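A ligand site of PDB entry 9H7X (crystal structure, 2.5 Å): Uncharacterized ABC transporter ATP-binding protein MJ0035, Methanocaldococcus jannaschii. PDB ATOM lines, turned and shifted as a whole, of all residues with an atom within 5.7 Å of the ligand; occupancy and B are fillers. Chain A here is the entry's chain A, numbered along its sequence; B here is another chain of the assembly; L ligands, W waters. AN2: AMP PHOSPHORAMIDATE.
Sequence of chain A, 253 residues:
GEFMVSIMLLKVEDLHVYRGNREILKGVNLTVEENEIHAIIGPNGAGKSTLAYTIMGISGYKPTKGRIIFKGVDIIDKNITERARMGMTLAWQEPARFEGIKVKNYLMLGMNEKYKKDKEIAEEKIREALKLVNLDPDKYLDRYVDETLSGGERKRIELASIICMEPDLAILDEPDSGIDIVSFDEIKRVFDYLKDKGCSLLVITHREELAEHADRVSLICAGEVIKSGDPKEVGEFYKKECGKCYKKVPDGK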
ATOM      1  N   ARG A  19     -25.610  15.846   6.124  1.00  0.00           N
ATOM      2  CA  ARG A  19     -24.202  15.890   6.496  1.00  0.00           C
ATOM      3  C   ARG A  19     -23.509  16.959   5.682  1.00  0.00           C
ATOM      4  O   ARG A  19     -23.507  16.886   4.451  1.00  0.00           O
ATOM      5  CB  ARG A  19     -23.525  14.518   6.352  1.00  0.00           C
ATOM      6  CG  ARG A  19     -23.925  13.544   7.451  1.00  0.00           C
ATOM      7  CD  ARG A  19     -23.364  13.972   8.794  1.00  0.00           C
ATOM      8  NE  ARG A  19     -21.909  13.856   8.812  1.00  0.00           N
ATOM      9  CZ  ARG A  19     -21.120  14.364   9.767  1.00  0.00           C
ATOM     10  NH1 ARG A  19     -21.646  15.022  10.782  1.00  0.00           N
ATOM     11  NH2 ARG A  19     -19.805  14.206   9.689  1.00  0.00           N
ATOM     12  N   GLY A  20     -22.988  17.967   6.361  1.00  0.00           N
ATOM     13  CA  GLY A  20     -22.334  19.092   5.735  1.00  0.00           C
ATOM     14  C   GLY A  20     -23.315  19.908   4.925  1.00  0.00           C
ATOM     15  O   GLY A  20     -24.049  20.740   5.475  1.00  0.00           O
ATOM     16  N   ASN A  21     -23.366  19.660   3.623  1.00  0.00           N
ATOM     17  CA  ASN A  21     -24.264  20.355   2.726  1.00  0.00           C
ATOM     18  C   ASN A  21     -25.317  19.386   2.160  1.00  0.00           C
ATOM     19  O   ASN A  21     -26.497  19.725   2.093  1.00  0.00           O
ATOM     20  CB  ASN A  21     -23.447  20.981   1.589  1.00  0.00           C
ATOM     21  CG  ASN A  21     -24.213  21.968   0.752  1.00  0.00           C
ATOM     22  OD1 ASN A  21     -25.271  22.487   1.155  1.00  0.00           O
ATOM     23  ND2 ASN A  21     -23.681  22.262  -0.426  1.00  0.00           N
ATOM     24  N   ARG A  22     -24.875  18.186   1.762  1.00  0.00           N
ATOM     25  CA  ARG A  22     -25.681  17.140   1.142  1.00  0.00           C
ATOM     26  C   ARG A  22     -26.693  16.503   2.114  1.00  0.00           C
ATOM     27  O   ARG A  22     -26.466  16.470   3.319  1.00  0.00           O
ATOM     28  CB  ARG A  22     -24.751  16.067   0.558  1.00  0.00           C
ATOM     29  CG  ARG A  22     -25.320  15.276  -0.617  1.00  0.00           C
ATOM     30  CD  ARG A  22     -24.251  14.892  -1.631  1.00  0.00           C
ATOM     31  NE  ARG A  22     -23.203  14.053  -1.051  1.00  0.00           N
ATOM     32  CZ  ARG A  22     -22.139  13.603  -1.722  1.00  0.00           C
ATOM     33  NH1 ARG A  22     -21.974  13.913  -3.006  1.00  0.00           N
ATOM     34  NH2 ARG A  22     -21.232  12.851  -1.112  1.00  0.00           N
ATOM     35  N   ILE A  24     -27.992  13.174   3.157  1.00  0.00           N
ATOM     36  CA  ILE A  24     -27.578  11.791   3.034  1.00  0.00           C
ATOM     37  C   ILE A  24     -28.755  10.831   3.219  1.00  0.00           C
ATOM     38  O   ILE A  24     -29.010  10.019   2.317  1.00  0.00           O
ATOM     39  CB  ILE A  24     -26.366  11.477   3.957  1.00  0.00           C
ATOM     40  CG1 ILE A  24     -25.081  12.012   3.315  1.00  0.00           C
ATOM     41  CG2 ILE A  24     -26.209   9.980   4.199  1.00  0.00           C
ATOM     42  CD1 ILE A  24     -24.852  13.457   3.301  1.00  0.00           C
ATOM     43  N   GLY A  42     -26.072  -2.344   0.360  1.00  0.00           N
ATOM     44  CA  GLY A  42     -26.215  -1.183  -0.507  1.00  0.00           C
ATOM     45  C   GLY A  42     -24.891  -0.640  -0.989  1.00  0.00           C
ATOM     46  O   GLY A  42     -23.835  -0.960  -0.441  1.00  0.00           O
ATOM     47  N   PRO A  43     -24.958   0.210  -2.028  1.00  0.00           N
ATOM     48  CA  PRO A  43     -23.713   0.754  -2.613  1.00  0.00           C
ATOM     49  C   PRO A  43     -22.990   1.774  -1.748  1.00  0.00           C
ATOM     50  O   PRO A  43     -23.515   2.184  -0.710  1.00  0.00           O
ATOM     51  CB  PRO A  43     -24.197   1.360  -3.938  1.00  0.00           C
ATOM     52  CG  PRO A  43     -25.618   1.717  -3.696  1.00  0.00           C
ATOM     53  CD  PRO A  43     -26.153   0.647  -2.780  1.00  0.00           C
ATOM     54  N   ASN A  44     -21.775   2.177  -2.149  1.00  0.00           N
ATOM     55  CA  ASN A  44     -21.021   3.186  -1.426  1.00  0.00           C
ATOM     56  C   ASN A  44     -21.729   4.529  -1.541  1.00  0.00           C
ATOM     57  O   ASN A  44     -22.252   4.866  -2.595  1.00  0.00           O
ATOM     58  CB  ASN A  44     -19.614   3.340  -2.008  1.00  0.00           C
ATOM     59  CG  ASN A  44     -18.660   2.220  -1.679  1.00  0.00           C
ATOM     60  OD1 ASN A  44     -17.691   1.996  -2.408  1.00  0.00           O
ATOM     61  ND2 ASN A  44     -18.901   1.476  -0.613  1.00  0.00           N
ATOM     62  N   GLY A  45     -21.763   5.276  -0.443  1.00  0.00           N
ATOM     63  CA  GLY A  45     -22.403   6.581  -0.432  1.00  0.00           C
ATOM     64  C   GLY A  45     -23.902   6.568  -0.271  1.00  0.00           C
ATOM     65  O   GLY A  45     -24.519   7.628  -0.256  1.00  0.00           O
ATOM     66  N   ALA A  46     -24.506   5.370  -0.115  1.00  0.00           N
ATOM     67  CA  ALA A  46     -25.936   5.242   0.084  1.00  0.00           C
ATOM     68  C   ALA A  46     -26.426   5.719   1.485  1.00  0.00           C
ATOM     69  O   ALA A  46     -27.623   5.965   1.671  1.00  0.00           O
ATOM     70  CB  ALA A  46     -26.373   3.816  -0.186  1.00  0.00           C
ATOM     71  N   GLY A  47     -25.525   5.837   2.439  1.00  0.00           N
ATOM     72  CA  GLY A  47     -25.855   6.334   3.764  1.00  0.00           C
ATOM     73  C   GLY A  47     -25.955   5.292   4.863  1.00  0.00           C
ATOM     74  O   GLY A  47     -26.441   5.603   5.951  1.00  0.00           O
ATOM     75  N   LYS A  48     -25.489   4.069   4.604  1.00  0.00           N
ATOM     76  CA  LYS A  48     -25.548   2.988   5.583  1.00  0.00           C
ATOM     77  C   LYS A  48     -24.777   3.304   6.870  1.00  0.00           C
ATOM     78  O   LYS A  48     -25.338   3.183   7.951  1.00  0.00           O
ATOM     79  CB  LYS A  48     -25.092   1.654   4.978  1.00  0.00           C
ATOM     80  CG  LYS A  48     -25.697   1.362   3.603  1.00  0.00           C
ATOM     81  CD  LYS A  48     -25.257   0.019   3.064  1.00  0.00           C
ATOM     82  CE  LYS A  48     -23.776  -0.068   2.818  1.00  0.00           C
ATOM     83  NZ  LYS A  48     -23.325   0.960   1.834  1.00  0.00           N
ATOM     84  N   SER A  49     -23.513   3.758   6.764  1.00  0.00           N
ATOM     85  CA  SER A  49     -22.708   4.144   7.923  1.00  0.00           C
ATOM     86  C   SER A  49     -23.330   5.334   8.615  1.00  0.00           C
ATOM     87  O   SER A  49     -23.401   5.341   9.829  1.00  0.00           O
ATOM     88  CB  SER A  49     -21.274   4.510   7.525  1.00  0.00           C
ATOM     89  OG  SER A  49     -20.489   3.363   7.261  1.00  0.00           O
ATOM     90  N   THR A  50     -23.854   6.297   7.853  1.00  0.00           N
ATOM     91  CA  THR A  50     -24.503   7.466   8.432  1.00  0.00           C
ATOM     92  C   THR A  50     -25.714   7.055   9.273  1.00  0.00           C
ATOM     93  O   THR A  50     -25.907   7.597  10.351  1.00  0.00           O
ATOM     94  CB  THR A  50     -24.817   8.500   7.347  1.00  0.00           C
ATOM     95  OG1 THR A  50     -23.576   8.942   6.775  1.00  0.00           O
ATOM     96  CG2 THR A  50     -25.609   9.695   7.871  1.00  0.00           C
ATOM     97  N   LEU A  51     -26.454   6.038   8.819  1.00  0.00           N
ATOM     98  CA  LEU A  51     -27.589   5.513   9.570  1.00  0.00           C
ATOM     99  C   LEU A  51     -27.123   4.935  10.894  1.00  0.00           C
ATOM    100  O   LEU A  51     -27.726   5.235  11.920  1.00  0.00           O
ATOM    101  CB  LEU A  51     -28.338   4.446   8.750  1.00  0.00           C
ATOM    102  CG  LEU A  51     -29.491   3.740   9.465  1.00  0.00           C
ATOM    103  CD1 LEU A  51     -30.555   4.719   9.867  1.00  0.00           C
ATOM    104  CD2 LEU A  51     -30.061   2.625   8.627  1.00  0.00           C
ATOM    105  N   TYR A  61     -24.235  13.836  14.032  1.00  0.00           N
ATOM    106  CA  TYR A  61     -25.241  13.067  13.316  1.00  0.00           C
ATOM    107  C   TYR A  61     -26.632  13.241  13.924  1.00  0.00           C
ATOM    108  O   TYR A  61     -27.202  12.290  14.465  1.00  0.00           O
ATOM    109  CB  TYR A  61     -24.833  11.592  13.235  1.00  0.00           C
ATOM    110  CG  TYR A  61     -23.626  11.367  12.350  1.00  0.00           C
ATOM    111  CD1 TYR A  61     -22.348  11.600  12.823  1.00  0.00           C
ATOM    112  CD2 TYR A  61     -23.762  10.938  11.050  1.00  0.00           C
ATOM    113  CE1 TYR A  61     -21.236  11.411  12.023  1.00  0.00           C
ATOM    114  CE2 TYR A  61     -22.654  10.721  10.237  1.00  0.00           C
ATOM    115  CZ  TYR A  61     -21.393  10.973  10.723  1.00  0.00           C
ATOM    116  OH  TYR A  61     -20.287  10.766   9.939  1.00  0.00           O
ATOM    117  N   ASP A 173     -20.643  -2.210  11.812  1.00  0.00           N
ATOM    118  CA  ASP A 173     -20.347  -1.628  10.510  1.00  0.00           C
ATOM    119  C   ASP A 173     -19.193  -2.410   9.878  1.00  0.00           C
ATOM    120  O   ASP A 173     -18.032  -2.215  10.236  1.00  0.00           O
ATOM    121  CB  ASP A 173     -19.962  -0.143  10.689  1.00  0.00           C
ATOM    122  CG  ASP A 173     -19.814   0.645   9.397  1.00  0.00           C
ATOM    123  OD1 ASP A 173     -20.246   0.130   8.341  1.00  0.00           O
ATOM    124  OD2 ASP A 173     -19.286   1.778   9.458  1.00  0.00           O
ATOM    125  N   ILE A 204     -24.055  -4.040   8.936  1.00  0.00           N
ATOM    126  CA  ILE A 204     -23.841  -3.473   7.620  1.00  0.00           C
ATOM    127  C   ILE A 204     -22.756  -4.343   6.991  1.00  0.00           C
ATOM    128  O   ILE A 204     -21.711  -4.540   7.613  1.00  0.00           O
ATOM    129  CB  ILE A 204     -23.377  -2.011   7.710  1.00  0.00           C
ATOM    130  CG1 ILE A 204     -24.488  -1.114   8.210  1.00  0.00           C
ATOM    131  CG2 ILE A 204     -22.825  -1.523   6.371  1.00  0.00           C
ATOM    132  CD1 ILE A 204     -24.020   0.154   8.643  1.00  0.00           C
ATOM    133  N   HIS A 206     -20.833  -6.056   3.070  1.00  0.00           N
ATOM    134  CA  HIS A 206     -20.602  -6.215   1.638  1.00  0.00           C
ATOM    135  C   HIS A 206     -20.368  -7.703   1.256  1.00  0.00           C
ATOM    136  O   HIS A 206     -20.225  -8.017   0.071  1.00  0.00           O
ATOM    137  CB  HIS A 206     -19.463  -5.312   1.118  1.00  0.00           C
ATOM    138  CG  HIS A 206     -19.811  -3.847   1.050  1.00  0.00           C
ATOM    139  ND1 HIS A 206     -20.638  -3.329   0.061  1.00  0.00           N
ATOM    140  CD2 HIS A 206     -19.434  -2.830   1.860  1.00  0.00           C
ATOM    141  CE1 HIS A 206     -20.734  -2.033   0.311  1.00  0.00           C
ATOM    142  NE2 HIS A 206     -20.032  -1.690   1.380  1.00  0.00           N
ATOM    143  N   TYR B 140     -16.358  15.704  -6.321  1.00  0.00           N
ATOM    144  CA  TYR B 140     -15.297  15.345  -5.397  1.00  0.00           C
ATOM    145  C   TYR B 140     -13.998  16.136  -5.478  1.00  0.00           C
ATOM    146  O   TYR B 140     -13.217  16.018  -4.539  1.00  0.00           O
ATOM    147  CB  TYR B 140     -14.977  13.852  -5.524  1.00  0.00           C
ATOM    148  CG  TYR B 140     -16.100  12.961  -5.059  1.00  0.00           C
ATOM    149  CD1 TYR B 140     -16.216  12.583  -3.726  1.00  0.00           C
ATOM    150  CD2 TYR B 140     -17.062  12.499  -5.942  1.00  0.00           C
ATOM    151  CE1 TYR B 140     -17.246  11.763  -3.298  1.00  0.00           C
ATOM    152  CE2 TYR B 140     -18.099  11.681  -5.527  1.00  0.00           C
ATOM    153  CZ  TYR B 140     -18.181  11.315  -4.194  1.00  0.00           C
ATOM    154  OH  TYR B 140     -19.213  10.511  -3.762  1.00  0.00           O
ATOM    155  N   ARG B 143     -13.814  18.460  -2.516  1.00  0.00           N
ATOM    156  CA  ARG B 143     -13.945  17.818  -1.219  1.00  0.00           C
ATOM    157  C   ARG B 143     -12.574  17.664  -0.548  1.00  0.00           C
ATOM    158  O   ARG B 143     -11.545  17.785  -1.199  1.00  0.00           O
ATOM    159  CB  ARG B 143     -14.640  16.459  -1.357  1.00  0.00           C
ATOM    160  CG  ARG B 143     -16.125  16.577  -1.612  1.00  0.00           C
ATOM    161  CD  ARG B 143     -16.927  16.817  -0.340  1.00  0.00           C
ATOM    162  NE  ARG B 143     -16.853  15.709   0.608  1.00  0.00           N
ATOM    163  CZ  ARG B 143     -17.533  14.570   0.491  1.00  0.00           C
ATOM    164  NH1 ARG B 143     -18.317  14.365  -0.570  1.00  0.00           N
ATOM    165  NH2 ARG B 143     -17.418  13.618   1.399  1.00  0.00           N
ATOM    166  N   THR B 148     -14.577  13.300   6.501  1.00  0.00           N
ATOM    167  CA  THR B 148     -15.832  13.545   5.842  1.00  0.00           C
ATOM    168  C   THR B 148     -16.140  12.501   4.749  1.00  0.00           C
ATOM    169  O   THR B 148     -17.300  12.179   4.521  1.00  0.00           O
ATOM    170  CB  THR B 148     -15.784  14.986   5.385  1.00  0.00           C
ATOM    171  OG1 THR B 148     -16.652  15.730   6.229  1.00  0.00           O
ATOM    172  CG2 THR B 148     -16.053  15.208   3.897  1.00  0.00           C
ATOM    173  N   LEU B 149     -15.109  11.967   4.104  1.00  0.00           N
ATOM    174  CA  LEU B 149     -15.281  10.947   3.081  1.00  0.00           C
ATOM    175  C   LEU B 149     -15.657   9.607   3.682  1.00  0.00           C
ATOM    176  O   LEU B 149     -15.147   9.255   4.740  1.00  0.00           O
ATOM    177  CB  LEU B 149     -13.951  10.751   2.348  1.00  0.00           C
ATOM    178  CG  LEU B 149     -13.447  11.904   1.548  1.00  0.00           C
ATOM    179  CD1 LEU B 149     -12.083  11.579   0.991  1.00  0.00           C
ATOM    180  CD2 LEU B 149     -14.402  12.251   0.415  1.00  0.00           C
ATOM    181  N   SER B 150     -16.482   8.820   2.969  1.00  0.00           N
ATOM    182  CA  SER B 150     -16.776   7.463   3.414  1.00  0.00           C
ATOM    183  C   SER B 150     -15.568   6.575   3.059  1.00  0.00           C
ATOM    184  O   SER B 150     -14.751   6.944   2.214  1.00  0.00           O
ATOM    185  CB  SER B 150     -18.082   6.947   2.792  1.00  0.00           C
ATOM    186  OG  SER B 150     -17.956   6.355   1.511  1.00  0.00           O
ATOM    187  N   GLY B 151     -15.451   5.434   3.715  1.00  0.00           N
ATOM    188  CA  GLY B 151     -14.339   4.522   3.465  1.00  0.00           C
ATOM    189  C   GLY B 151     -14.181   4.098   2.011  1.00  0.00           C
ATOM    190  O   GLY B 151     -13.069   3.998   1.499  1.00  0.00           O
ATOM    191  N   GLU B 153     -15.221   5.842  -0.630  1.00  0.00           N
ATOM    192  CA  GLU B 153     -14.775   7.022  -1.359  1.00  0.00           C
ATOM    193  C   GLU B 153     -13.296   7.255  -1.153  1.00  0.00           C
ATOM    194  O   GLU B 153     -12.593   7.559  -2.103  1.00  0.00           O
ATOM    195  CB  GLU B 153     -15.560   8.257  -0.912  1.00  0.00           C
ATOM    196  CG  GLU B 153     -17.021   8.163  -1.240  1.00  0.00           C
ATOM    197  CD  GLU B 153     -17.856   9.269  -0.636  1.00  0.00           C
ATOM    198  OE1 GLU B 153     -17.461   9.793   0.434  1.00  0.00           O
ATOM    199  OE2 GLU B 153     -18.906   9.614  -1.225  1.00  0.00           O
HETATM  200  N3B AN2 L   1     -21.804   3.675   4.539  1.00  0.00           N
HETATM  201  PB  AN2 L   1     -22.228   4.220   2.922  1.00  0.00           P
HETATM  202  O2B AN2 L   1     -20.981   3.813   2.233  1.00  0.00           O
HETATM  203  O1B AN2 L   1     -23.508   3.495   2.802  1.00  0.00           O
HETATM  204  O3A AN2 L   1     -22.352   5.841   3.099  1.00  0.00           O
HETATM  205  PA  AN2 L   1     -21.946   6.968   4.161  1.00  0.00           P
HETATM  206  O1A AN2 L   1     -23.139   7.295   4.969  1.00  0.00           O
HETATM  207  O2A AN2 L   1     -20.659   6.642   4.820  1.00  0.00           O
HETATM  208  O5' AN2 L   1     -21.695   8.213   3.208  1.00  0.00           O
HETATM  209  C5' AN2 L   1     -22.775   9.110   2.945  1.00  0.00           C
HETATM  210  C4' AN2 L   1     -22.268  10.291   2.158  1.00  0.00           C
HETATM  211  O4' AN2 L   1     -22.132  11.443   3.014  1.00  0.00           O
HETATM  212  C3' AN2 L   1     -20.914  10.108   1.454  1.00  0.00           C
HETATM  213  O3' AN2 L   1     -21.054  10.229   0.046  1.00  0.00           O
HETATM  214  C2' AN2 L   1     -20.030  11.211   2.084  1.00  0.00           C
HETATM  215  O2' AN2 L   1     -19.087  11.749   1.171  1.00  0.00           O
HETATM  216  C1' AN2 L   1     -21.085  12.215   2.509  1.00  0.00           C
HETATM  217  N9  AN2 L   1     -20.660  13.145   3.546  1.00  0.00           N
HETATM  218  C8  AN2 L   1     -20.497  12.879   4.880  1.00  0.00           C
HETATM  219  N7  AN2 L   1     -20.154  13.926   5.591  1.00  0.00           N
HETATM  220  C5  AN2 L   1     -20.075  14.945   4.647  1.00  0.00           C
HETATM  221  C4  AN2 L   1     -20.386  14.474   3.386  1.00  0.00           C
HETATM  222  N3  AN2 L   1     -20.394  15.183   2.254  1.00  0.00           N
HETATM  223  C2  AN2 L   1     -20.043  16.454   2.473  1.00  0.00           C
HETATM  224  N1  AN2 L   1     -19.710  17.037   3.622  1.00  0.00           N
HETATM  225  C6  AN2 L   1     -19.721  16.306   4.760  1.00  0.00           C
HETATM  226  N6  AN2 L   1     -19.457  16.921   5.912  1.00  0.00           N
HETATM  227  O   HOH W   1     -18.431   3.275   2.593  1.00  0.00           O
HETATM  228  O   HOH W   2     -19.401  20.114   2.705  1.00  0.00           O
HETATM  229  O   HOH W   3     -20.500   1.425   1.712  1.00  0.00           O
HETATM  230  O   HOH W   4     -18.558   4.374   5.283  1.00  0.00           O
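O1A of the ligand is in hydrogen-bond range of N of Thr 50 (3.1 Å). An oxygen (O1A) of the ligand sits at hydrogen-bond distance from the side-chain hydroxyl (OG1) of Thr 50 (2.5 Å). The guanidinium group of Arg 143 of chain B lies within hydrogen-bond range of an oxygen (O2') of the ligand (2.5 Å). The side-chain carboxylate (OE2) of Glu 153 of chain B is in hydrogen-bond range of an oxygen (O3') of the ligand, 2.6 Å away. An oxygen (O1B) of the ligand sits at hydrogen-bond distance from the backbone NH of Lys 48 (2.7 Å). NZ of Lys 48 lies within salt-bridge range of O1B of the ligand (2.7 Å). A nitrogen (N3B) of the ligand sits at hydrogen-bond distance from the side-chain hydroxyl (OG) of Ser 49, 3.0 Å away. An oxygen (O3') of the ligand is in hydrogen-bond range of the guanidinium group (NH2) of Arg 22 (2.9 Å). The side-chain hydroxyl of Thr 148 of chain B is in hydrogen-bond range of a nitrogen (N6) of the ligand. The backbone NH (N) of Gly 47 sits at hydrogen-bond distance from an oxygen (O1B) of the ligand. The backbone NH of Gly 45 is in hydrogen-bond range of an oxygen (O2B) of the ligand, at 3.1 Å.
The side-chain carboxylate (OE1) of Glu 153 of chain B lies within salt-bridge range of the guanidinium group (NH2) of Arg 143 of chain B, at 3.9 Å. NH2 of Arg 143 of chain B sits close to O of Thr 148 of chain B, at 3.4 Å. The side-chain carboxylate (OE2) of Glu 153 of chain B lies within salt-bridge range of the guanidinium group (NH2) of Arg 22. The side-chain carboxylate (OE1) of Glu 153 of chain B lies within hydrogen-bond range of the backbone NH (N) of Ser 150 of chain B (2.9 Å). The side-chain carboxylate of Glu 153 of chain B is in hydrogen-bond range of the side-chain hydroxyl of Tyr 140 of chain B, at 2.7 Å. NZ of Lys 48 sits at hydrogen-bond distance from O of Pro 43. The side-chain amino group (NZ) of Lys 48 sits at hydrogen-bond distance from the backbone carbonyl oxygen (O) of Gly 42 (3.0 Å). The side-chain carboxylate (OD2) of Asp 173 sits at hydrogen-bond distance from the side-chain hydroxyl (OG) of Ser 49, 3.0 Å away.
Arg 19 touches the ligand. Gly 20 touches the ligand (CA to N6, 3.6 Å). CG1 of Ile 24 touches O4' of the ligand, at 3.0 Å. Pro 43 touches the ligand (O to O1B, 3.7 Å). Asn 44 touches the ligand (CA to O2B, 3.7 Å). Ala 46 touches the ligand. Ser 150 of chain B touches the ligand. Hydrophobic or aromatic side chains that line the ligand: Ile 24.
Water W3 lies within hydrogen-bond range of an oxygen (O2B) of the ligand (2.5 Å), the side-chain amide nitrogen (ND2) of Asn 44 (2.8 Å), the side-chain amino group (NZ) of Lys 48 (2.9 Å) and a ring nitrogen (NE2) of His 206 (3.2 Å). Water W1 bridges O2B of the ligand (2.6 Å) and OG of Ser 150 of chain B (3.3 Å). Water W4 lies within hydrogen-bond range of OG of Ser 49 (2.9 Å) and O2A of the ligand (3.1 Å).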
